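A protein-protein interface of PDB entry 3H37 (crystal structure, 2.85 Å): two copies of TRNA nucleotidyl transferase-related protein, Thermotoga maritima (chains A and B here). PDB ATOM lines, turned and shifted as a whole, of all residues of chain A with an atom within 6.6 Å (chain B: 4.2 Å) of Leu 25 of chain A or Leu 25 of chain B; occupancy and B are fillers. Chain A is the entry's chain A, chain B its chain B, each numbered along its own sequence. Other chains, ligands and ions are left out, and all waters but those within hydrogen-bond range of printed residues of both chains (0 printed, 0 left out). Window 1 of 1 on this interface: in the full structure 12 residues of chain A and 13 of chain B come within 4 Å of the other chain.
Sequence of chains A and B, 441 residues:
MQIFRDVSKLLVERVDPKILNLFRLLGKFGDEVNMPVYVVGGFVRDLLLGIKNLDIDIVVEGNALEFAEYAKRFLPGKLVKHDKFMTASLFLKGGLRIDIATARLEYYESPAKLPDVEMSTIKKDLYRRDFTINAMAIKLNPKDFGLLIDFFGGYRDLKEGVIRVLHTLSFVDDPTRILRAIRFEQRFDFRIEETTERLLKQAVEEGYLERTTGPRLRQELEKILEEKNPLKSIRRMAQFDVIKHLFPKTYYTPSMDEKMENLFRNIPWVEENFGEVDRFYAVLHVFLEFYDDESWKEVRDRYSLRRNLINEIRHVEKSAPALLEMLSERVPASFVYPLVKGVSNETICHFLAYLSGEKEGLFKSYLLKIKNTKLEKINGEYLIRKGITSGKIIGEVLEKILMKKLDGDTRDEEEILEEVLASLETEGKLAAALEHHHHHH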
ATOM      1  N   LEU A  20     -33.679  22.695  14.731  1.00  0.00           N
ATOM      2  CA  LEU A  20     -33.851  21.425  15.439  1.00  0.00           C
ATOM      3  C   LEU A  20     -33.046  20.292  14.813  1.00  0.00           C
ATOM      4  O   LEU A  20     -32.248  19.645  15.495  1.00  0.00           O
ATOM      5  CB  LEU A  20     -35.318  21.012  15.474  1.00  0.00           C
ATOM      6  CG  LEU A  20     -36.023  20.964  16.828  1.00  0.00           C
ATOM      7  CD1 LEU A  20     -37.417  20.402  16.637  1.00  0.00           C
ATOM      8  CD2 LEU A  20     -35.243  20.119  17.816  1.00  0.00           C
ATOM      9  N   ASN A  21     -33.252  20.041  13.523  1.00  0.00           N
ATOM     10  CA  ASN A  21     -32.476  19.001  12.852  1.00  0.00           C
ATOM     11  C   ASN A  21     -30.989  19.250  13.046  1.00  0.00           C
ATOM     12  O   ASN A  21     -30.173  18.330  13.075  1.00  0.00           O
ATOM     13  CB  ASN A  21     -32.813  18.924  11.364  1.00  0.00           C
ATOM     14  CG  ASN A  21     -34.239  18.476  11.113  1.00  0.00           C
ATOM     15  OD1 ASN A  21     -34.756  18.638  10.011  1.00  0.00           O
ATOM     16  ND2 ASN A  21     -34.888  17.908  12.136  1.00  0.00           N
ATOM     17  N   LEU A  22     -30.646  20.517  13.208  1.00  0.00           N
ATOM     18  CA  LEU A  22     -29.261  20.896  13.397  1.00  0.00           C
ATOM     19  C   LEU A  22     -28.828  20.449  14.780  1.00  0.00           C
ATOM     20  O   LEU A  22     -27.740  19.901  14.957  1.00  0.00           O
ATOM     21  CB  LEU A  22     -29.119  22.400  13.249  1.00  0.00           C
ATOM     22  CG  LEU A  22     -27.992  22.845  12.339  1.00  0.00           C
ATOM     23  CD1 LEU A  22     -27.801  24.343  12.477  1.00  0.00           C
ATOM     24  CD2 LEU A  22     -26.726  22.104  12.698  1.00  0.00           C
ATOM     25  N   PHE A  23     -29.699  20.671  15.757  1.00  0.00           N
ATOM     26  CA  PHE A  23     -29.419  20.272  17.126  1.00  0.00           C
ATOM     27  C   PHE A  23     -29.325  18.753  17.179  1.00  0.00           C
ATOM     28  O   PHE A  23     -28.434  18.189  17.815  1.00  0.00           O
ATOM     29  CB  PHE A  23     -30.521  20.761  18.075  1.00  0.00           C
ATOM     30  CG  PHE A  23     -30.459  22.230  18.402  1.00  0.00           C
ATOM     31  CD1 PHE A  23     -29.267  22.827  18.780  1.00  0.00           C
ATOM     32  CD2 PHE A  23     -31.608  23.002  18.376  1.00  0.00           C
ATOM     33  CE1 PHE A  23     -29.216  24.177  19.104  1.00  0.00           C
ATOM     34  CE2 PHE A  23     -31.557  24.350  18.700  1.00  0.00           C
ATOM     35  CZ  PHE A  23     -30.358  24.933  19.059  1.00  0.00           C
ATOM     36  N   ARG A  24     -30.261  18.094  16.514  1.00  0.00           N
ATOM     37  CA  ARG A  24     -30.272  16.645  16.469  1.00  0.00           C
ATOM     38  C   ARG A  24     -28.945  16.180  15.934  1.00  0.00           C
ATOM     39  O   ARG A  24     -28.254  15.367  16.554  1.00  0.00           O
ATOM     40  CB  ARG A  24     -31.384  16.164  15.552  1.00  0.00           C
ATOM     41  CG  ARG A  24     -32.704  15.945  16.257  1.00  0.00           C
ATOM     42  CD  ARG A  24     -33.874  16.226  15.337  1.00  0.00           C
ATOM     43  NE  ARG A  24     -35.152  15.993  15.999  1.00  0.00           N
ATOM     44  CZ  ARG A  24     -36.308  16.485  15.570  1.00  0.00           C
ATOM     45  NH1 ARG A  24     -36.328  17.250  14.481  1.00  0.00           N
ATOM     46  NH2 ARG A  24     -37.432  16.212  16.230  1.00  0.00           N
ATOM     47  N   LEU A  25     -28.589  16.709  14.770  1.00  0.00           N
ATOM     48  CA  LEU A  25     -27.390  16.264  14.091  1.00  0.00           C
ATOM     49  C   LEU A  25     -26.145  16.534  14.929  1.00  0.00           C
ATOM     50  O   LEU A  25     -25.268  15.665  15.045  1.00  0.00           O
ATOM     51  CB  LEU A  25     -27.298  16.906  12.716  1.00  0.00           C
ATOM     52  CG  LEU A  25     -28.191  16.253  11.659  1.00  0.00           C
ATOM     53  CD1 LEU A  25     -27.880  16.774  10.275  1.00  0.00           C
ATOM     54  CD2 LEU A  25     -28.060  14.735  11.677  1.00  0.00           C
ATOM     55  N   LEU A  26     -26.078  17.722  15.533  1.00  0.00           N
ATOM     56  CA  LEU A  26     -24.920  18.094  16.338  1.00  0.00           C
ATOM     57  C   LEU A  26     -24.714  17.089  17.462  1.00  0.00           C
ATOM     58  O   LEU A  26     -23.602  16.607  17.685  1.00  0.00           O
ATOM     59  CB  LEU A  26     -25.071  19.504  16.901  1.00  0.00           C
ATOM     60  CG  LEU A  26     -24.830  20.670  15.940  1.00  0.00           C
ATOM     61  CD1 LEU A  26     -24.979  22.049  16.652  1.00  0.00           C
ATOM     62  CD2 LEU A  26     -23.464  20.494  15.270  1.00  0.00           C
ATOM     63  N   GLY A  27     -25.799  16.761  18.162  1.00  0.00           N
ATOM     64  CA  GLY A  27     -25.730  15.774  19.224  1.00  0.00           C
ATOM     65  C   GLY A  27     -25.226  14.425  18.741  1.00  0.00           C
ATOM     66  O   GLY A  27     -24.306  13.845  19.339  1.00  0.00           O
ATOM     67  N   LYS A  28     -25.833  13.935  17.659  1.00  0.00           N
ATOM     68  CA  LYS A  28     -25.457  12.664  17.067  1.00  0.00           C
ATOM     69  C   LYS A  28     -23.957  12.635  16.806  1.00  0.00           C
ATOM     70  O   LYS A  28     -23.274  11.696  17.256  1.00  0.00           O
ATOM     71  CB  LYS A  28     -26.216  12.442  15.761  1.00  0.00           C
ATOM     72  CG  LYS A  28     -26.737  11.012  15.572  1.00  0.00           C
ATOM     73  CD  LYS A  28     -25.762   9.988  16.092  1.00  0.00           C
ATOM     74  CE  LYS A  28     -26.053   8.631  15.540  1.00  0.00           C
ATOM     75  NZ  LYS A  28     -24.751   8.038  15.100  1.00  0.00           N
ATOM     76  N   PHE A  29     -23.454  13.663  16.096  1.00  0.00           N
ATOM     77  CA  PHE A  29     -22.034  13.765  15.765  1.00  0.00           C
ATOM     78  C   PHE A  29     -21.213  13.639  17.018  1.00  0.00           C
ATOM     79  O   PHE A  29     -20.116  13.081  16.989  1.00  0.00           O
ATOM     80  CB  PHE A  29     -21.692  15.115  15.166  1.00  0.00           C
ATOM     81  CG  PHE A  29     -22.395  15.408  13.892  1.00  0.00           C
ATOM     82  CD1 PHE A  29     -22.597  16.716  13.493  1.00  0.00           C
ATOM     83  CD2 PHE A  29     -22.853  14.379  13.088  1.00  0.00           C
ATOM     84  CE1 PHE A  29     -23.248  16.994  12.322  1.00  0.00           C
ATOM     85  CE2 PHE A  29     -23.507  14.650  11.914  1.00  0.00           C
ATOM     86  CZ  PHE A  29     -23.713  15.956  11.536  1.00  0.00           C
ATOM     87  N   GLY A  30     -21.730  14.196  18.114  1.00  0.00           N
ATOM     88  CA  GLY A  30     -21.054  14.101  19.391  1.00  0.00           C
ATOM     89  C   GLY A  30     -20.832  12.657  19.790  1.00  0.00           C
ATOM     90  O   GLY A  30     -19.727  12.257  20.175  1.00  0.00           O
ATOM     91  N   GLU A  32     -20.751  10.194  17.864  1.00  0.00           N
ATOM     92  CA  GLU A  32     -19.817   9.611  16.908  1.00  0.00           C
ATOM     93  C   GLU A  32     -18.349   9.865  17.272  1.00  0.00           C
ATOM     94  O   GLU A  32     -17.487   9.060  16.942  1.00  0.00           O
ATOM     95  CB  GLU A  32     -20.149  10.063  15.480  1.00  0.00           C
ATOM     96  CG  GLU A  32     -21.587   9.757  15.099  1.00  0.00           C
ATOM     97  CD  GLU A  32     -21.978  10.230  13.713  1.00  0.00           C
ATOM     98  OE1 GLU A  32     -23.167  10.056  13.367  1.00  0.00           O
ATOM     99  OE2 GLU A  32     -21.115  10.766  12.975  1.00  0.00           O
ATOM    100  N   PHE A  67     -14.183  18.582  17.095  1.00  0.00           N
ATOM    101  CA  PHE A  67     -15.619  18.535  16.877  1.00  0.00           C
ATOM    102  C   PHE A  67     -16.028  19.299  15.622  1.00  0.00           C
ATOM    103  O   PHE A  67     -16.631  18.718  14.715  1.00  0.00           O
ATOM    104  CB  PHE A  67     -16.390  19.073  18.087  1.00  0.00           C
ATOM    105  CG  PHE A  67     -17.883  18.951  17.947  1.00  0.00           C
ATOM    106  CD1 PHE A  67     -18.517  17.744  18.201  1.00  0.00           C
ATOM    107  CD2 PHE A  67     -18.647  20.032  17.525  1.00  0.00           C
ATOM    108  CE1 PHE A  67     -19.883  17.618  18.050  1.00  0.00           C
ATOM    109  CE2 PHE A  67     -20.018  19.906  17.379  1.00  0.00           C
ATOM    110  CZ  PHE A  67     -20.634  18.699  17.635  1.00  0.00           C
ATOM    111  N   PHE A  74     -20.085  16.924   7.241  1.00  0.00           N
ATOM    112  CA  PHE A  74     -21.485  16.577   7.010  1.00  0.00           C
ATOM    113  C   PHE A  74     -22.371  17.811   6.910  1.00  0.00           C
ATOM    114  O   PHE A  74     -23.447  17.780   6.313  1.00  0.00           O
ATOM    115  CB  PHE A  74     -21.967  15.632   8.115  1.00  0.00           C
ATOM    116  CG  PHE A  74     -21.049  14.479   8.334  1.00  0.00           C
ATOM    117  CD1 PHE A  74     -20.234  14.427   9.450  1.00  0.00           C
ATOM    118  CD2 PHE A  74     -20.949  13.476   7.383  1.00  0.00           C
ATOM    119  CE1 PHE A  74     -19.361  13.367   9.639  1.00  0.00           C
ATOM    120  CE2 PHE A  74     -20.080  12.421   7.565  1.00  0.00           C
ATOM    121  CZ  PHE A  74     -19.283  12.365   8.693  1.00  0.00           C
ATOM    122  N   LEU A  75     -21.895  18.904   7.491  1.00  0.00           N
ATOM    123  CA  LEU A  75     -22.577  20.182   7.418  1.00  0.00           C
ATOM    124  C   LEU A  75     -21.897  21.087   6.388  1.00  0.00           C
ATOM    125  O   LEU A  75     -20.674  21.229   6.389  1.00  0.00           O
ATOM    126  CB  LEU A  75     -22.588  20.843   8.800  1.00  0.00           C
ATOM    127  CG  LEU A  75     -23.755  20.523   9.747  1.00  0.00           C
ATOM    128  CD1 LEU A  75     -24.576  19.325   9.284  1.00  0.00           C
ATOM    129  CD2 LEU A  75     -23.242  20.316  11.160  1.00  0.00           C
ATOM    130  N   PHE A 145     -31.392  14.203  24.964  1.00  0.00           N
ATOM    131  CA  PHE A 145     -31.535  15.323  24.087  1.00  0.00           C
ATOM    132  C   PHE A 145     -32.251  16.572  24.560  1.00  0.00           C
ATOM    133  O   PHE A 145     -31.606  17.605  24.619  1.00  0.00           O
ATOM    134  CB  PHE A 145     -32.179  14.820  22.799  1.00  0.00           C
ATOM    135  CG  PHE A 145     -32.413  15.877  21.785  1.00  0.00           C
ATOM    136  CD1 PHE A 145     -33.673  16.328  21.528  1.00  0.00           C
ATOM    137  CD2 PHE A 145     -31.375  16.417  21.084  1.00  0.00           C
ATOM    138  CE1 PHE A 145     -33.886  17.289  20.604  1.00  0.00           C
ATOM    139  CE2 PHE A 145     -31.598  17.379  20.176  1.00  0.00           C
ATOM    140  CZ  PHE A 145     -32.851  17.814  19.933  1.00  0.00           C
ATOM    141  N   ASN B  21     -27.037  11.900   6.695  1.00  0.00           N
ATOM    142  CA  ASN B  21     -27.644  12.782   7.674  1.00  0.00           C
ATOM    143  C   ASN B  21     -29.086  12.424   7.859  1.00  0.00           C
ATOM    144  O   ASN B  21     -29.584  12.356   8.977  1.00  0.00           O
ATOM    145  CB  ASN B  21     -27.535  14.233   7.218  1.00  0.00           C
ATOM    146  CG  ASN B  21     -26.279  14.896   7.717  1.00  0.00           C
ATOM    147  OD1 ASN B  21     -25.490  14.285   8.442  1.00  0.00           O
ATOM    148  ND2 ASN B  21     -26.083  16.155   7.338  1.00  0.00           N
ATOM    149  N   LEU B  22     -29.754  12.217   6.735  1.00  0.00           N
ATOM    150  CA  LEU B  22     -31.119  11.734   6.718  1.00  0.00           C
ATOM    151  C   LEU B  22     -31.222  10.412   7.479  1.00  0.00           C
ATOM    152  O   LEU B  22     -32.203  10.168   8.174  1.00  0.00           O
ATOM    153  CB  LEU B  22     -31.576  11.565   5.282  1.00  0.00           C
ATOM    154  CG  LEU B  22     -33.062  11.405   5.053  1.00  0.00           C
ATOM    155  CD1 LEU B  22     -33.842  12.155   6.118  1.00  0.00           C
ATOM    156  CD2 LEU B  22     -33.375  11.950   3.683  1.00  0.00           C
ATOM    157  N   PHE B  23     -30.201   9.564   7.373  1.00  0.00           N
ATOM    158  CA  PHE B  23     -30.202   8.317   8.140  1.00  0.00           C
ATOM    159  C   PHE B  23     -30.169   8.573   9.636  1.00  0.00           C
ATOM    160  O   PHE B  23     -30.906   7.928  10.382  1.00  0.00           O
ATOM    161  CB  PHE B  23     -29.051   7.393   7.748  1.00  0.00           C
ATOM    162  CG  PHE B  23     -29.298   6.635   6.486  1.00  0.00           C
ATOM    163  CD1 PHE B  23     -30.594   6.445   6.022  1.00  0.00           C
ATOM    164  CD2 PHE B  23     -28.240   6.086   5.768  1.00  0.00           C
ATOM    165  CE1 PHE B  23     -30.828   5.741   4.855  1.00  0.00           C
ATOM    166  CE2 PHE B  23     -28.469   5.384   4.603  1.00  0.00           C
ATOM    167  CZ  PHE B  23     -29.763   5.209   4.147  1.00  0.00           C
ATOM    168  N   ARG B  24     -29.305   9.499  10.061  1.00  0.00           N
ATOM    169  CA  ARG B  24     -29.163   9.880  11.472  1.00  0.00           C
ATOM    170  C   ARG B  24     -30.450  10.498  12.007  1.00  0.00           C
ATOM    171  O   ARG B  24     -30.900  10.193  13.119  1.00  0.00           O
ATOM    172  CB  ARG B  24     -28.054  10.903  11.634  1.00  0.00           C
ATOM    173  CG  ARG B  24     -26.655  10.455  11.278  1.00  0.00           C
ATOM    174  CD  ARG B  24     -25.736  11.610  11.613  1.00  0.00           C
ATOM    175  NE  ARG B  24     -24.310  11.333  11.481  1.00  0.00           N
ATOM    176  CZ  ARG B  24     -23.573  11.648  10.415  1.00  0.00           C
ATOM    177  NH1 ARG B  24     -24.134  12.223   9.350  1.00  0.00           N
ATOM    178  NH2 ARG B  24     -22.274  11.375  10.415  1.00  0.00           N
ATOM    179  N   LEU B  25     -31.029  11.378  11.196  1.00  0.00           N
ATOM    180  CA  LEU B  25     -32.273  12.027  11.539  1.00  0.00           C
ATOM    181  C   LEU B  25     -33.391  11.007  11.712  1.00  0.00           C
ATOM    182  O   LEU B  25     -34.013  10.939  12.776  1.00  0.00           O
ATOM    183  CB  LEU B  25     -32.644  13.063  10.477  1.00  0.00           C
ATOM    184  CG  LEU B  25     -31.914  14.404  10.553  1.00  0.00           C
ATOM    185  CD1 LEU B  25     -32.678  15.447   9.771  1.00  0.00           C
ATOM    186  CD2 LEU B  25     -31.759  14.852  12.001  1.00  0.00           C
ATOM    187  N   LEU B  26     -33.645  10.224  10.661  1.00  0.00           N
ATOM    188  CA  LEU B  26     -34.668   9.183  10.693  1.00  0.00           C
ATOM    189  C   LEU B  26     -34.526   8.323  11.938  1.00  0.00           C
ATOM    190  O   LEU B  26     -35.513   8.047  12.618  1.00  0.00           O
ATOM    191  CB  LEU B  26     -34.593   8.325   9.443  1.00  0.00           C
ATOM    192  CG  LEU B  26     -35.287   8.971   8.241  1.00  0.00           C
ATOM    193  CD1 LEU B  26     -35.229   8.069   7.006  1.00  0.00           C
ATOM    194  CD2 LEU B  26     -36.719   9.313   8.621  1.00  0.00           C
ATOM    195  N   GLY B  27     -33.298   7.930  12.260  1.00  0.00           N
ATOM    196  CA  GLY B  27     -33.050   7.188  13.482  1.00  0.00           C
ATOM    197  C   GLY B  27     -33.429   7.943  14.748  1.00  0.00           C
ATOM    198  O   GLY B  27     -33.861   7.340  15.731  1.00  0.00           O
ATOM    199  N   LYS B  28     -33.257   9.265  14.728  1.00  0.00           N
ATOM    200  CA  LYS B  28     -33.560  10.095  15.890  1.00  0.00           C
ATOM    201  C   LYS B  28     -35.074  10.233  16.060  1.00  0.00           C
ATOM    202  O   LYS B  28     -35.608  10.053  17.156  1.00  0.00           O
ATOM    203  CB  LYS B  28     -32.898  11.467  15.761  1.00  0.00           C
ATOM    204  CG  LYS B  28     -32.265  11.982  17.041  1.00  0.00           C
ATOM    205  CD  LYS B  28     -33.253  11.994  18.191  1.00  0.00           C
ATOM    206  CE  LYS B  28     -32.766  12.822  19.351  1.00  0.00           C
ATOM    207  NZ  LYS B  28     -33.905  13.041  20.273  1.00  0.00           N
ATOM    208  N   PHE B  29     -35.769  10.548  14.974  1.00  0.00           N
ATOM    209  CA  PHE B  29     -37.218  10.479  14.995  1.00  0.00           C
ATOM    210  C   PHE B  29     -37.655   9.137  15.594  1.00  0.00           C
ATOM    211  O   PHE B  29     -38.571   9.074  16.415  1.00  0.00           O
ATOM    212  CB  PHE B  29     -37.776  10.608  13.585  1.00  0.00           C
ATOM    213  CG  PHE B  29     -37.378  11.867  12.894  1.00  0.00           C
ATOM    214  CD1 PHE B  29     -37.480  11.970  11.516  1.00  0.00           C
ATOM    215  CD2 PHE B  29     -36.897  12.949  13.618  1.00  0.00           C
ATOM    216  CE1 PHE B  29     -37.118  13.125  10.865  1.00  0.00           C
ATOM    217  CE2 PHE B  29     -36.528  14.111  12.975  1.00  0.00           C
ATOM    218  CZ  PHE B  29     -36.639  14.198  11.590  1.00  0.00           C
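Among the printed residues, merely in contact across the chains: Phe 29 of chain A with Arg 24 of chain B, Arg 24 of chain A with Phe 29 of chain B, Leu 25 of chain A with Asn 21 of chain B, Phe 145 of chain A with Lys 28 of chain B, Phe 74 of chain A with Arg 24 of chain B, Asn 21 of chain A with Leu 25 of chain B, Leu 25 of chain A with Leu 25 of chain B, Arg 24 of chain A with Leu 25 of chain B, Leu 25 of chain A with Arg 24 of chain B and Phe 29 of chain A with Asn 21 of chain B.
The side-chain amide oxygen (OD1) of Asn 21 of chain B lies within hydrogen-bond range of the guanidinium group (NH1) of Arg 24 of chain B, 2.6 Å away. The side-chain amide nitrogen (ND2) of Asn 21 of chain A lies close to the guanidinium group (NH1) of Arg 24 of chain A (2.8 Å). NZ of Lys 28 of chain A is in salt-bridge range of OE1 of Glu 32 of chain A (3.1 Å).
NE of Arg 24 of chain B is in salt-bridge range of OE1 of Glu 32 of chain A (2.5 Å). The backbone carbonyl oxygen (O) of Phe 74 of chain A is in hydrogen-bond range of the side-chain amide nitrogen (ND2) of Asn 21 of chain B.
Of the printed residues of chain B, Leu 25 of chain A touches Asn 21, Arg 24 and Leu 25. Of chain A, only Asn 21 (3.7 Å), Arg 24 (3.8 Å) and Leu 25 (3.7 Å) come within 4 Å of Leu 25 of chain B. Of the printed residues of chain B, Arg 24 of chain A touches Leu 25 and Phe 29. Of the printed residues of chain B, Phe 29 of chain A touches Asn 21 and Arg 24. Printed residues of chain B within 4 Å of Asn 21 of chain A: Leu 25 (3.7 Å). Of the printed residues of chain B, Glu 32 of chain A touches Arg 24 (2.5 Å). The nearest printed residue of chain B that does not touch Leu 25 of chain A is Leu 22 of chain B (5.8 Å). The nearest residue of chain A that does not touch Leu 25 of chain B is Leu 22 of chain A (5.9 Å). The nearest printed residue of chain B that does not touch Phe 145 of chain A is Leu 25 of chain B (8.5 Å).
Asn 21 of chain A touches Leu 25 of chain B, and with the chains exchanged Leu 25 of chain A touches Asn 21 of chain B. Arg 24 of chain A touches Phe 29 of chain B, and with the chains exchanged Phe 29 of chain A touches Arg 24 of chain B. Leu 25 of chain A touches its own counterpart, Leu 25 of chain B. Phe 29 of chain A touches Asn 21 of chain B, but with the chains exchanged Asn 21 of chain A does not touch Phe 29 of chain B (4.1 Å). Positions printed for both chains: 21, 22, 23, 24, 25, 26, 27, 28 and 29. Of the 12 pairs that touch across the chains among the printed residues, 7 have their exchanged pair printed and touching as well.
Hydrophobic or aromatic side chains of chain B within 4 Å of the printed part of chain A: Leu 25 and Phe 29.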
